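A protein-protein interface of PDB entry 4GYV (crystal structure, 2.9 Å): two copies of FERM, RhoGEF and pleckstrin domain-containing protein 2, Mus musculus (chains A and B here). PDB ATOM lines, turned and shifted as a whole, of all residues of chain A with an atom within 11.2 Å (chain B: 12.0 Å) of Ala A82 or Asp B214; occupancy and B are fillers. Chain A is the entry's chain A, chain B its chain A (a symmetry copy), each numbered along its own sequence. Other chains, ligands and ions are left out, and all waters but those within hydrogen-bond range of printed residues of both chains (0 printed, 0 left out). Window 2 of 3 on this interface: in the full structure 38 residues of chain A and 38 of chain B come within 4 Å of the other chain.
The side-chain carboxylate (OE1) of Glu B210 is in hydrogen-bond range of the backbone NH (N) of Gly A1, at 2.7 Å.
The backbone NH of Ala A82 sits at hydrogen-bond distance from the side-chain carboxylate of Asp B214, 3.0 Å away.
The side-chain carboxylate (OE2) of Glu B210 is in salt-bridge range of the side-chain amino group (NZ) of Lys A85, at 3.8 Å.
O of Gly A1 is in hydrogen-bond range of NE2 of Gln A89, at 3.3 Å.
The side-chain hydroxyl (OG) of Ser A80 is in hydrogen-bond range of the backbone carbonyl oxygen (O) of Leu A75, at 3.2 Å.
The backbone carbonyl oxygen (O) of Gly A78 lies within hydrogen-bond range of the side-chain hydroxyl (OG) of Ser A80 (3.1 Å).
OG of Ser A80 is in hydrogen-bond range of ND1 of His A88 (3.3 Å).
OE1 of Glu B210 sits close to OE1 of Gln B206, 3.2 Å away.
Among the printed residues, pairs that only touch across the chains: Pro A79 with Pro B145 (3.7 Å), Ser A80 with Asp B214 (3.8 Å) and Ser A81 with Asp B214 (3.7 Å).
Ala A82 touches one residue of chain B.
Of the printed residues of chain A, Asp B214 touches Ser A80, Ser A81 and Ala A82.
Of chain B, only Asp B214 (3.7 Å) comes within 4 Å of Ser A81.
No residue of chain B comes within 4 Å of Leu A84.
Lys A85 touches one residue of chain B.
Arg B213 touches none of the printed residues of chain A.
Printed residues of chain A within 4 Å of Glu B210: Gly A1 (2.7 Å) and Lys A85 (3.8 Å).
Of the printed residues of chain B, Gly A1 touches Glu B210.
Of the printed residues of chain B, Pro A79 touches Pro B145.
Of the printed residues of chain A, Pro B145 touches Pro A79 (3.7 Å).
Gly A78 touches none of the printed residues of chain B.
Of the 13 printed residues of chain B, 3 touch a printed residue of chain A.
Among the printed residues, Asp or Glu carboxylates within 4 Å of a Lys or Arg side-chain nitrogen of the other chain: Lys A85 with Glu B210.
No position is printed for both chains.
Of the 6 pairs that touch across the chains among the printed residues, none has its exchanged pair printed and touching as well.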
ATOM      1  N   GLY A   1     -24.881   3.736 -25.955  1.00  0.00           N
ATOM      2  CA  GLY A   1     -25.147   5.165 -25.978  1.00  0.00           C
ATOM      3  C   GLY A   1     -26.605   5.501 -26.248  1.00  0.00           C
ATOM      4  O   GLY A   1     -27.463   4.626 -26.170  1.00  0.00           O
ATOM      5  N   LEU A  75     -24.674   7.878 -17.719  1.00  0.00           N
ATOM      6  CA  LEU A  75     -25.103   6.498 -17.812  1.00  0.00           C
ATOM      7  C   LEU A  75     -25.842   6.262 -19.124  1.00  0.00           C
ATOM      8  O   LEU A  75     -25.736   5.197 -19.745  1.00  0.00           O
ATOM      9  CB  LEU A  75     -25.999   6.149 -16.632  1.00  0.00           C
ATOM     10  CG  LEU A  75     -25.279   5.865 -15.322  1.00  0.00           C
ATOM     11  CD1 LEU A  75     -26.273   5.462 -14.295  1.00  0.00           C
ATOM     12  CD2 LEU A  75     -24.292   4.792 -15.522  1.00  0.00           C
ATOM     13  N   GLY A  78     -23.242   6.464 -21.946  1.00  0.00           N
ATOM     14  CA  GLY A  78     -22.297   5.360 -21.894  1.00  0.00           C
ATOM     15  C   GLY A  78     -22.886   3.983 -22.109  1.00  0.00           C
ATOM     16  O   GLY A  78     -24.104   3.815 -22.165  1.00  0.00           O
ATOM     17  N   PRO A  79     -22.020   2.975 -22.219  1.00  0.00           N
ATOM     18  CA  PRO A  79     -22.487   1.623 -22.549  1.00  0.00           C
ATOM     19  C   PRO A  79     -23.186   1.014 -21.341  1.00  0.00           C
ATOM     20  O   PRO A  79     -22.717   1.136 -20.213  1.00  0.00           O
ATOM     21  CB  PRO A  79     -21.194   0.877 -22.859  1.00  0.00           C
ATOM     22  CG  PRO A  79     -20.180   1.536 -21.982  1.00  0.00           C
ATOM     23  CD  PRO A  79     -20.583   2.999 -21.899  1.00  0.00           C
ATOM     24  N   SER A  80     -24.326   0.387 -21.566  1.00  0.00           N
ATOM     25  CA  SER A  80     -25.110  -0.080 -20.453  1.00  0.00           C
ATOM     26  C   SER A  80     -25.436  -1.531 -20.718  1.00  0.00           C
ATOM     27  O   SER A  80     -25.700  -1.918 -21.868  1.00  0.00           O
ATOM     28  CB  SER A  80     -26.397   0.752 -20.327  1.00  0.00           C
ATOM     29  OG  SER A  80     -26.193   2.163 -20.508  1.00  0.00           O
ATOM     30  N   SER A  81     -25.380  -2.345 -19.666  1.00  0.00           N
ATOM     31  CA  SER A  81     -25.837  -3.727 -19.756  1.00  0.00           C
ATOM     32  C   SER A  81     -27.298  -3.708 -20.147  1.00  0.00           C
ATOM     33  O   SER A  81     -28.033  -2.823 -19.720  1.00  0.00           O
ATOM     34  CB  SER A  81     -25.686  -4.438 -18.418  1.00  0.00           C
ATOM     35  OG  SER A  81     -24.329  -4.706 -18.135  1.00  0.00           O
ATOM     36  N   ALA A  82     -27.720  -4.675 -20.951  1.00  0.00           N
ATOM     37  CA  ALA A  82     -29.075  -4.674 -21.480  1.00  0.00           C
ATOM     38  C   ALA A  82     -30.137  -4.457 -20.408  1.00  0.00           C
ATOM     39  O   ALA A  82     -31.065  -3.669 -20.607  1.00  0.00           O
ATOM     40  CB  ALA A  82     -29.346  -5.947 -22.238  1.00  0.00           C
ATOM     41  N   HIS A  83     -29.996  -5.120 -19.265  1.00  0.00           N
ATOM     42  CA  HIS A  83     -31.005  -4.988 -18.214  1.00  0.00           C
ATOM     43  C   HIS A  83     -31.082  -3.599 -17.574  1.00  0.00           C
ATOM     44  O   HIS A  83     -32.066  -3.281 -16.925  1.00  0.00           O
ATOM     45  CB  HIS A  83     -30.837  -6.054 -17.140  1.00  0.00           C
ATOM     46  CG  HIS A  83     -29.606  -5.881 -16.318  1.00  0.00           C
ATOM     47  ND1 HIS A  83     -28.372  -6.328 -16.734  1.00  0.00           N
ATOM     48  CD2 HIS A  83     -29.416  -5.304 -15.109  1.00  0.00           C
ATOM     49  CE1 HIS A  83     -27.473  -6.029 -15.813  1.00  0.00           C
ATOM     50  NE2 HIS A  83     -28.081  -5.407 -14.818  1.00  0.00           N
ATOM     51  N   LEU A  84     -30.068  -2.762 -17.758  1.00  0.00           N
ATOM     52  CA  LEU A  84     -30.107  -1.417 -17.173  1.00  0.00           C
ATOM     53  C   LEU A  84     -30.405  -0.351 -18.207  1.00  0.00           C
ATOM     54  O   LEU A  84     -30.598   0.815 -17.861  1.00  0.00           O
ATOM     55  CB  LEU A  84     -28.782  -1.066 -16.492  1.00  0.00           C
ATOM     56  CG  LEU A  84     -28.207  -2.036 -15.469  1.00  0.00           C
ATOM     57  CD1 LEU A  84     -26.781  -1.688 -15.222  1.00  0.00           C
ATOM     58  CD2 LEU A  84     -28.985  -1.962 -14.201  1.00  0.00           C
ATOM     59  N   LYS A  85     -30.426  -0.762 -19.471  1.00  0.00           N
ATOM     60  CA  LYS A  85     -30.550   0.146 -20.605  1.00  0.00           C
ATOM     61  C   LYS A  85     -31.789   1.026 -20.477  1.00  0.00           C
ATOM     62  O   LYS A  85     -31.732   2.214 -20.729  1.00  0.00           O
ATOM     63  CB  LYS A  85     -30.548  -0.650 -21.916  1.00  0.00           C
ATOM     64  CG  LYS A  85     -29.898   0.052 -23.093  1.00  0.00           C
ATOM     65  CD  LYS A  85     -29.721  -0.886 -24.297  1.00  0.00           C
ATOM     66  CE  LYS A  85     -28.523  -1.838 -24.129  1.00  0.00           C
ATOM     67  NZ  LYS A  85     -27.800  -2.129 -25.427  1.00  0.00           N
ATOM     68  N   GLY A  86     -32.894   0.457 -20.035  1.00  0.00           N
ATOM     69  CA  GLY A  86     -34.113   1.220 -19.938  1.00  0.00           C
ATOM     70  C   GLY A  86     -34.160   2.216 -18.808  1.00  0.00           C
ATOM     71  O   GLY A  86     -34.782   3.265 -18.942  1.00  0.00           O
ATOM     72  N   ASP A  87     -33.507   1.876 -17.699  1.00  0.00           N
ATOM     73  CA  ASP A  87     -33.392   2.734 -16.520  1.00  0.00           C
ATOM     74  C   ASP A  87     -32.396   3.847 -16.721  1.00  0.00           C
ATOM     75  O   ASP A  87     -32.591   4.958 -16.222  1.00  0.00           O
ATOM     76  CB  ASP A  87     -32.943   1.917 -15.323  1.00  0.00           C
ATOM     77  CG  ASP A  87     -33.965   0.883 -14.924  1.00  0.00           C
ATOM     78  OD1 ASP A  87     -35.177   1.194 -15.050  1.00  0.00           O
ATOM     79  OD2 ASP A  87     -33.559  -0.231 -14.501  1.00  0.00           O
ATOM     80  N   HIS A  88     -31.317   3.539 -17.435  1.00  0.00           N
ATOM     81  CA  HIS A  88     -30.305   4.535 -17.757  1.00  0.00           C
ATOM     82  C   HIS A  88     -30.767   5.489 -18.831  1.00  0.00           C
ATOM     83  O   HIS A  88     -30.236   6.575 -18.944  1.00  0.00           O
ATOM     84  CB  HIS A  88     -29.004   3.880 -18.232  1.00  0.00           C
ATOM     85  CG  HIS A  88     -28.249   3.167 -17.155  1.00  0.00           C
ATOM     86  ND1 HIS A  88     -27.064   2.513 -17.394  1.00  0.00           N
ATOM     87  CD2 HIS A  88     -28.506   3.008 -15.836  1.00  0.00           C
ATOM     88  CE1 HIS A  88     -26.625   1.973 -16.272  1.00  0.00           C
ATOM     89  NE2 HIS A  88     -27.482   2.258 -15.310  1.00  0.00           N
ATOM     90  N   GLN A  89     -31.729   5.087 -19.653  1.00  0.00           N
ATOM     91  CA  GLN A  89     -32.079   5.933 -20.791  1.00  0.00           C
ATOM     92  C   GLN A  89     -33.379   6.689 -20.606  1.00  0.00           C
ATOM     93  O   GLN A  89     -34.276   6.679 -21.456  1.00  0.00           O
ATOM     94  CB  GLN A  89     -31.992   5.147 -22.081  1.00  0.00           C
ATOM     95  CG  GLN A  89     -30.543   4.842 -22.333  1.00  0.00           C
ATOM     96  CD  GLN A  89     -30.277   3.874 -23.443  1.00  0.00           C
ATOM     97  OE1 GLN A  89     -31.162   3.552 -24.228  1.00  0.00           O
ATOM     98  NE2 GLN A  89     -29.032   3.398 -23.520  1.00  0.00           N
ATOM     99  N   PRO B 145     -16.536   5.737 -23.636  1.00  0.00           N
ATOM    100  CA  PRO B 145     -15.536   5.077 -24.465  1.00  0.00           C
ATOM    101  C   PRO B 145     -15.180   6.002 -25.608  1.00  0.00           C
ATOM    102  O   PRO B 145     -16.071   6.595 -26.217  1.00  0.00           O
ATOM    103  CB  PRO B 145     -16.263   3.854 -24.982  1.00  0.00           C
ATOM    104  CG  PRO B 145     -17.512   3.730 -24.198  1.00  0.00           C
ATOM    105  CD  PRO B 145     -17.572   4.801 -23.185  1.00  0.00           C
ATOM    106  N   LEU B 205     -23.252   0.964 -36.692  1.00  0.00           N
ATOM    107  CA  LEU B 205     -21.966   0.706 -36.058  1.00  0.00           C
ATOM    108  C   LEU B 205     -21.960   0.744 -34.536  1.00  0.00           C
ATOM    109  O   LEU B 205     -21.307  -0.096 -33.910  1.00  0.00           O
ATOM    110  CB  LEU B 205     -20.907   1.669 -36.566  1.00  0.00           C
ATOM    111  CG  LEU B 205     -20.222   1.124 -37.808  1.00  0.00           C
ATOM    112  CD1 LEU B 205     -19.010   1.987 -38.117  1.00  0.00           C
ATOM    113  CD2 LEU B 205     -19.849  -0.354 -37.620  1.00  0.00           C
ATOM    114  N   GLN B 206     -22.648   1.715 -33.934  1.00  0.00           N
ATOM    115  CA  GLN B 206     -22.616   1.808 -32.473  1.00  0.00           C
ATOM    116  C   GLN B 206     -23.409   0.659 -31.909  1.00  0.00           C
ATOM    117  O   GLN B 206     -22.909  -0.087 -31.067  1.00  0.00           O
ATOM    118  CB  GLN B 206     -23.122   3.150 -31.922  1.00  0.00           C
ATOM    119  CG  GLN B 206     -24.583   3.487 -32.197  1.00  0.00           C
ATOM    120  CD  GLN B 206     -25.193   4.403 -31.155  1.00  0.00           C
ATOM    121  OE1 GLN B 206     -24.801   4.379 -29.985  1.00  0.00           O
ATOM    122  NE2 GLN B 206     -26.166   5.213 -31.575  1.00  0.00           N
ATOM    123  N   LYS B 207     -24.630   0.496 -32.408  1.00  0.00           N
ATOM    124  CA  LYS B 207     -25.479  -0.581 -31.954  1.00  0.00           C
ATOM    125  C   LYS B 207     -24.749  -1.928 -32.023  1.00  0.00           C
ATOM    126  O   LYS B 207     -24.837  -2.716 -31.087  1.00  0.00           O
ATOM    127  CB  LYS B 207     -26.792  -0.615 -32.731  1.00  0.00           C
ATOM    128  CG  LYS B 207     -27.804  -1.602 -32.159  1.00  0.00           C
ATOM    129  CD  LYS B 207     -28.896  -0.889 -31.409  1.00  0.00           C
ATOM    130  CE  LYS B 207     -29.688  -1.804 -30.506  1.00  0.00           C
ATOM    131  NZ  LYS B 207     -30.703  -0.980 -29.817  1.00  0.00           N
ATOM    132  N   LEU B 208     -23.998  -2.180 -33.094  1.00  0.00           N
ATOM    133  CA  LEU B 208     -23.244  -3.435 -33.174  1.00  0.00           C
ATOM    134  C   LEU B 208     -22.175  -3.517 -32.085  1.00  0.00           C
ATOM    135  O   LEU B 208     -21.871  -4.598 -31.571  1.00  0.00           O
ATOM    136  CB  LEU B 208     -22.611  -3.633 -34.550  1.00  0.00           C
ATOM    137  CG  LEU B 208     -21.715  -4.862 -34.700  1.00  0.00           C
ATOM    138  CD1 LEU B 208     -22.458  -6.112 -34.321  1.00  0.00           C
ATOM    139  CD2 LEU B 208     -21.202  -4.998 -36.109  1.00  0.00           C
ATOM    140  N   THR B 209     -21.616  -2.370 -31.713  1.00  0.00           N
ATOM    141  CA  THR B 209     -20.543  -2.388 -30.736  1.00  0.00           C
ATOM    142  C   THR B 209     -21.073  -2.638 -29.337  1.00  0.00           C
ATOM    143  O   THR B 209     -20.566  -3.508 -28.629  1.00  0.00           O
ATOM    144  CB  THR B 209     -19.742  -1.087 -30.708  1.00  0.00           C
ATOM    145  OG1 THR B 209     -19.531  -0.601 -32.041  1.00  0.00           O
ATOM    146  CG2 THR B 209     -18.412  -1.355 -30.041  1.00  0.00           C
ATOM    147  N   GLU B 210     -22.080  -1.859 -28.938  1.00  0.00           N
ATOM    148  CA  GLU B 210     -22.620  -1.962 -27.592  1.00  0.00           C
ATOM    149  C   GLU B 210     -23.261  -3.328 -27.410  1.00  0.00           C
ATOM    150  O   GLU B 210     -23.280  -3.870 -26.307  1.00  0.00           O
ATOM    151  CB  GLU B 210     -23.586  -0.808 -27.270  1.00  0.00           C
ATOM    152  CG  GLU B 210     -24.566  -0.441 -28.386  1.00  0.00           C
ATOM    153  CD  GLU B 210     -25.504   0.738 -28.040  1.00  0.00           C
ATOM    154  OE1 GLU B 210     -25.024   1.898 -27.934  1.00  0.00           O
ATOM    155  OE2 GLU B 210     -26.732   0.491 -27.895  1.00  0.00           O
ATOM    156  N   LEU B 211     -23.743  -3.894 -28.511  1.00  0.00           N
ATOM    157  CA  LEU B 211     -24.334  -5.219 -28.499  1.00  0.00           C
ATOM    158  C   LEU B 211     -23.287  -6.306 -28.402  1.00  0.00           C
ATOM    159  O   LEU B 211     -23.529  -7.372 -27.811  1.00  0.00           O
ATOM    160  CB  LEU B 211     -25.171  -5.450 -29.751  1.00  0.00           C
ATOM    161  CG  LEU B 211     -26.579  -4.860 -29.815  1.00  0.00           C
ATOM    162  CD1 LEU B 211     -27.309  -5.364 -31.060  1.00  0.00           C
ATOM    163  CD2 LEU B 211     -27.347  -5.186 -28.557  1.00  0.00           C
ATOM    164  N   GLN B 212     -22.131  -6.061 -29.007  1.00  0.00           N
ATOM    165  CA  GLN B 212     -21.087  -7.080 -29.024  1.00  0.00           C
ATOM    166  C   GLN B 212     -20.332  -7.061 -27.701  1.00  0.00           C
ATOM    167  O   GLN B 212     -19.868  -8.100 -27.217  1.00  0.00           O
ATOM    168  CB  GLN B 212     -20.148  -6.854 -30.204  1.00  0.00           C
ATOM    169  CG  GLN B 212     -19.581  -8.134 -30.803  1.00  0.00           C
ATOM    170  CD  GLN B 212     -19.038  -7.922 -32.213  1.00  0.00           C
ATOM    171  OE1 GLN B 212     -19.285  -6.886 -32.839  1.00  0.00           O
ATOM    172  NE2 GLN B 212     -18.296  -8.904 -32.714  1.00  0.00           N
ATOM    173  N   ARG B 213     -20.259  -5.860 -27.115  1.00  0.00           N
ATOM    174  CA  ARG B 213     -19.635  -5.611 -25.813  1.00  0.00           C
ATOM    175  C   ARG B 213     -20.387  -6.270 -24.652  1.00  0.00           C
ATOM    176  O   ARG B 213     -19.896  -6.301 -23.532  1.00  0.00           O
ATOM    177  CB  ARG B 213     -19.527  -4.085 -25.570  1.00  0.00           C
ATOM    178  N   ASP B 214     -21.566  -6.815 -24.936  1.00  0.00           N
ATOM    179  CA  ASP B 214     -22.529  -7.191 -23.908  1.00  0.00           C
ATOM    180  C   ASP B 214     -23.343  -8.425 -24.359  1.00  0.00           C
ATOM    181  O   ASP B 214     -24.483  -8.311 -24.805  1.00  0.00           O
ATOM    182  CB  ASP B 214     -23.413  -5.954 -23.641  1.00  0.00           C
ATOM    183  CG  ASP B 214     -24.553  -6.205 -22.656  1.00  0.00           C
ATOM    184  OD1 ASP B 214     -24.393  -6.955 -21.663  1.00  0.00           O
ATOM    185  OD2 ASP B 214     -25.630  -5.612 -22.885  1.00  0.00           O
ATOM    186  N   LEU B 215     -22.749  -9.605 -24.260  1.00  0.00           N
ATOM    187  CA  LEU B 215     -23.417 -10.823 -24.691  1.00  0.00           C
ATOM    188  C   LEU B 215     -23.701 -11.693 -23.489  1.00  0.00           C
ATOM    189  O   LEU B 215     -22.948 -11.651 -22.535  1.00  0.00           O
ATOM    190  CB  LEU B 215     -22.512 -11.613 -25.632  1.00  0.00           C
ATOM    191  CG  LEU B 215     -21.858 -10.961 -26.839  1.00  0.00           C
ATOM    192  CD1 LEU B 215     -20.783 -11.862 -27.346  1.00  0.00           C
ATOM    193  CD2 LEU B 215     -22.866 -10.728 -27.918  1.00  0.00           C
ATOM    194  N   VAL B 216     -24.750 -12.503 -23.512  1.00  0.00           N
ATOM    195  CA  VAL B 216     -24.982 -13.348 -22.366  1.00  0.00           C
ATOM    196  C   VAL B 216     -23.828 -14.317 -22.245  1.00  0.00           C
ATOM    197  O   VAL B 216     -23.223 -14.425 -21.185  1.00  0.00           O
ATOM    198  CB  VAL B 216     -26.292 -14.129 -22.462  1.00  0.00           C
ATOM    199  CG1 VAL B 216     -27.437 -13.193 -22.604  1.00  0.00           C
ATOM    200  CG2 VAL B 216     -26.247 -15.092 -23.628  1.00  0.00           C
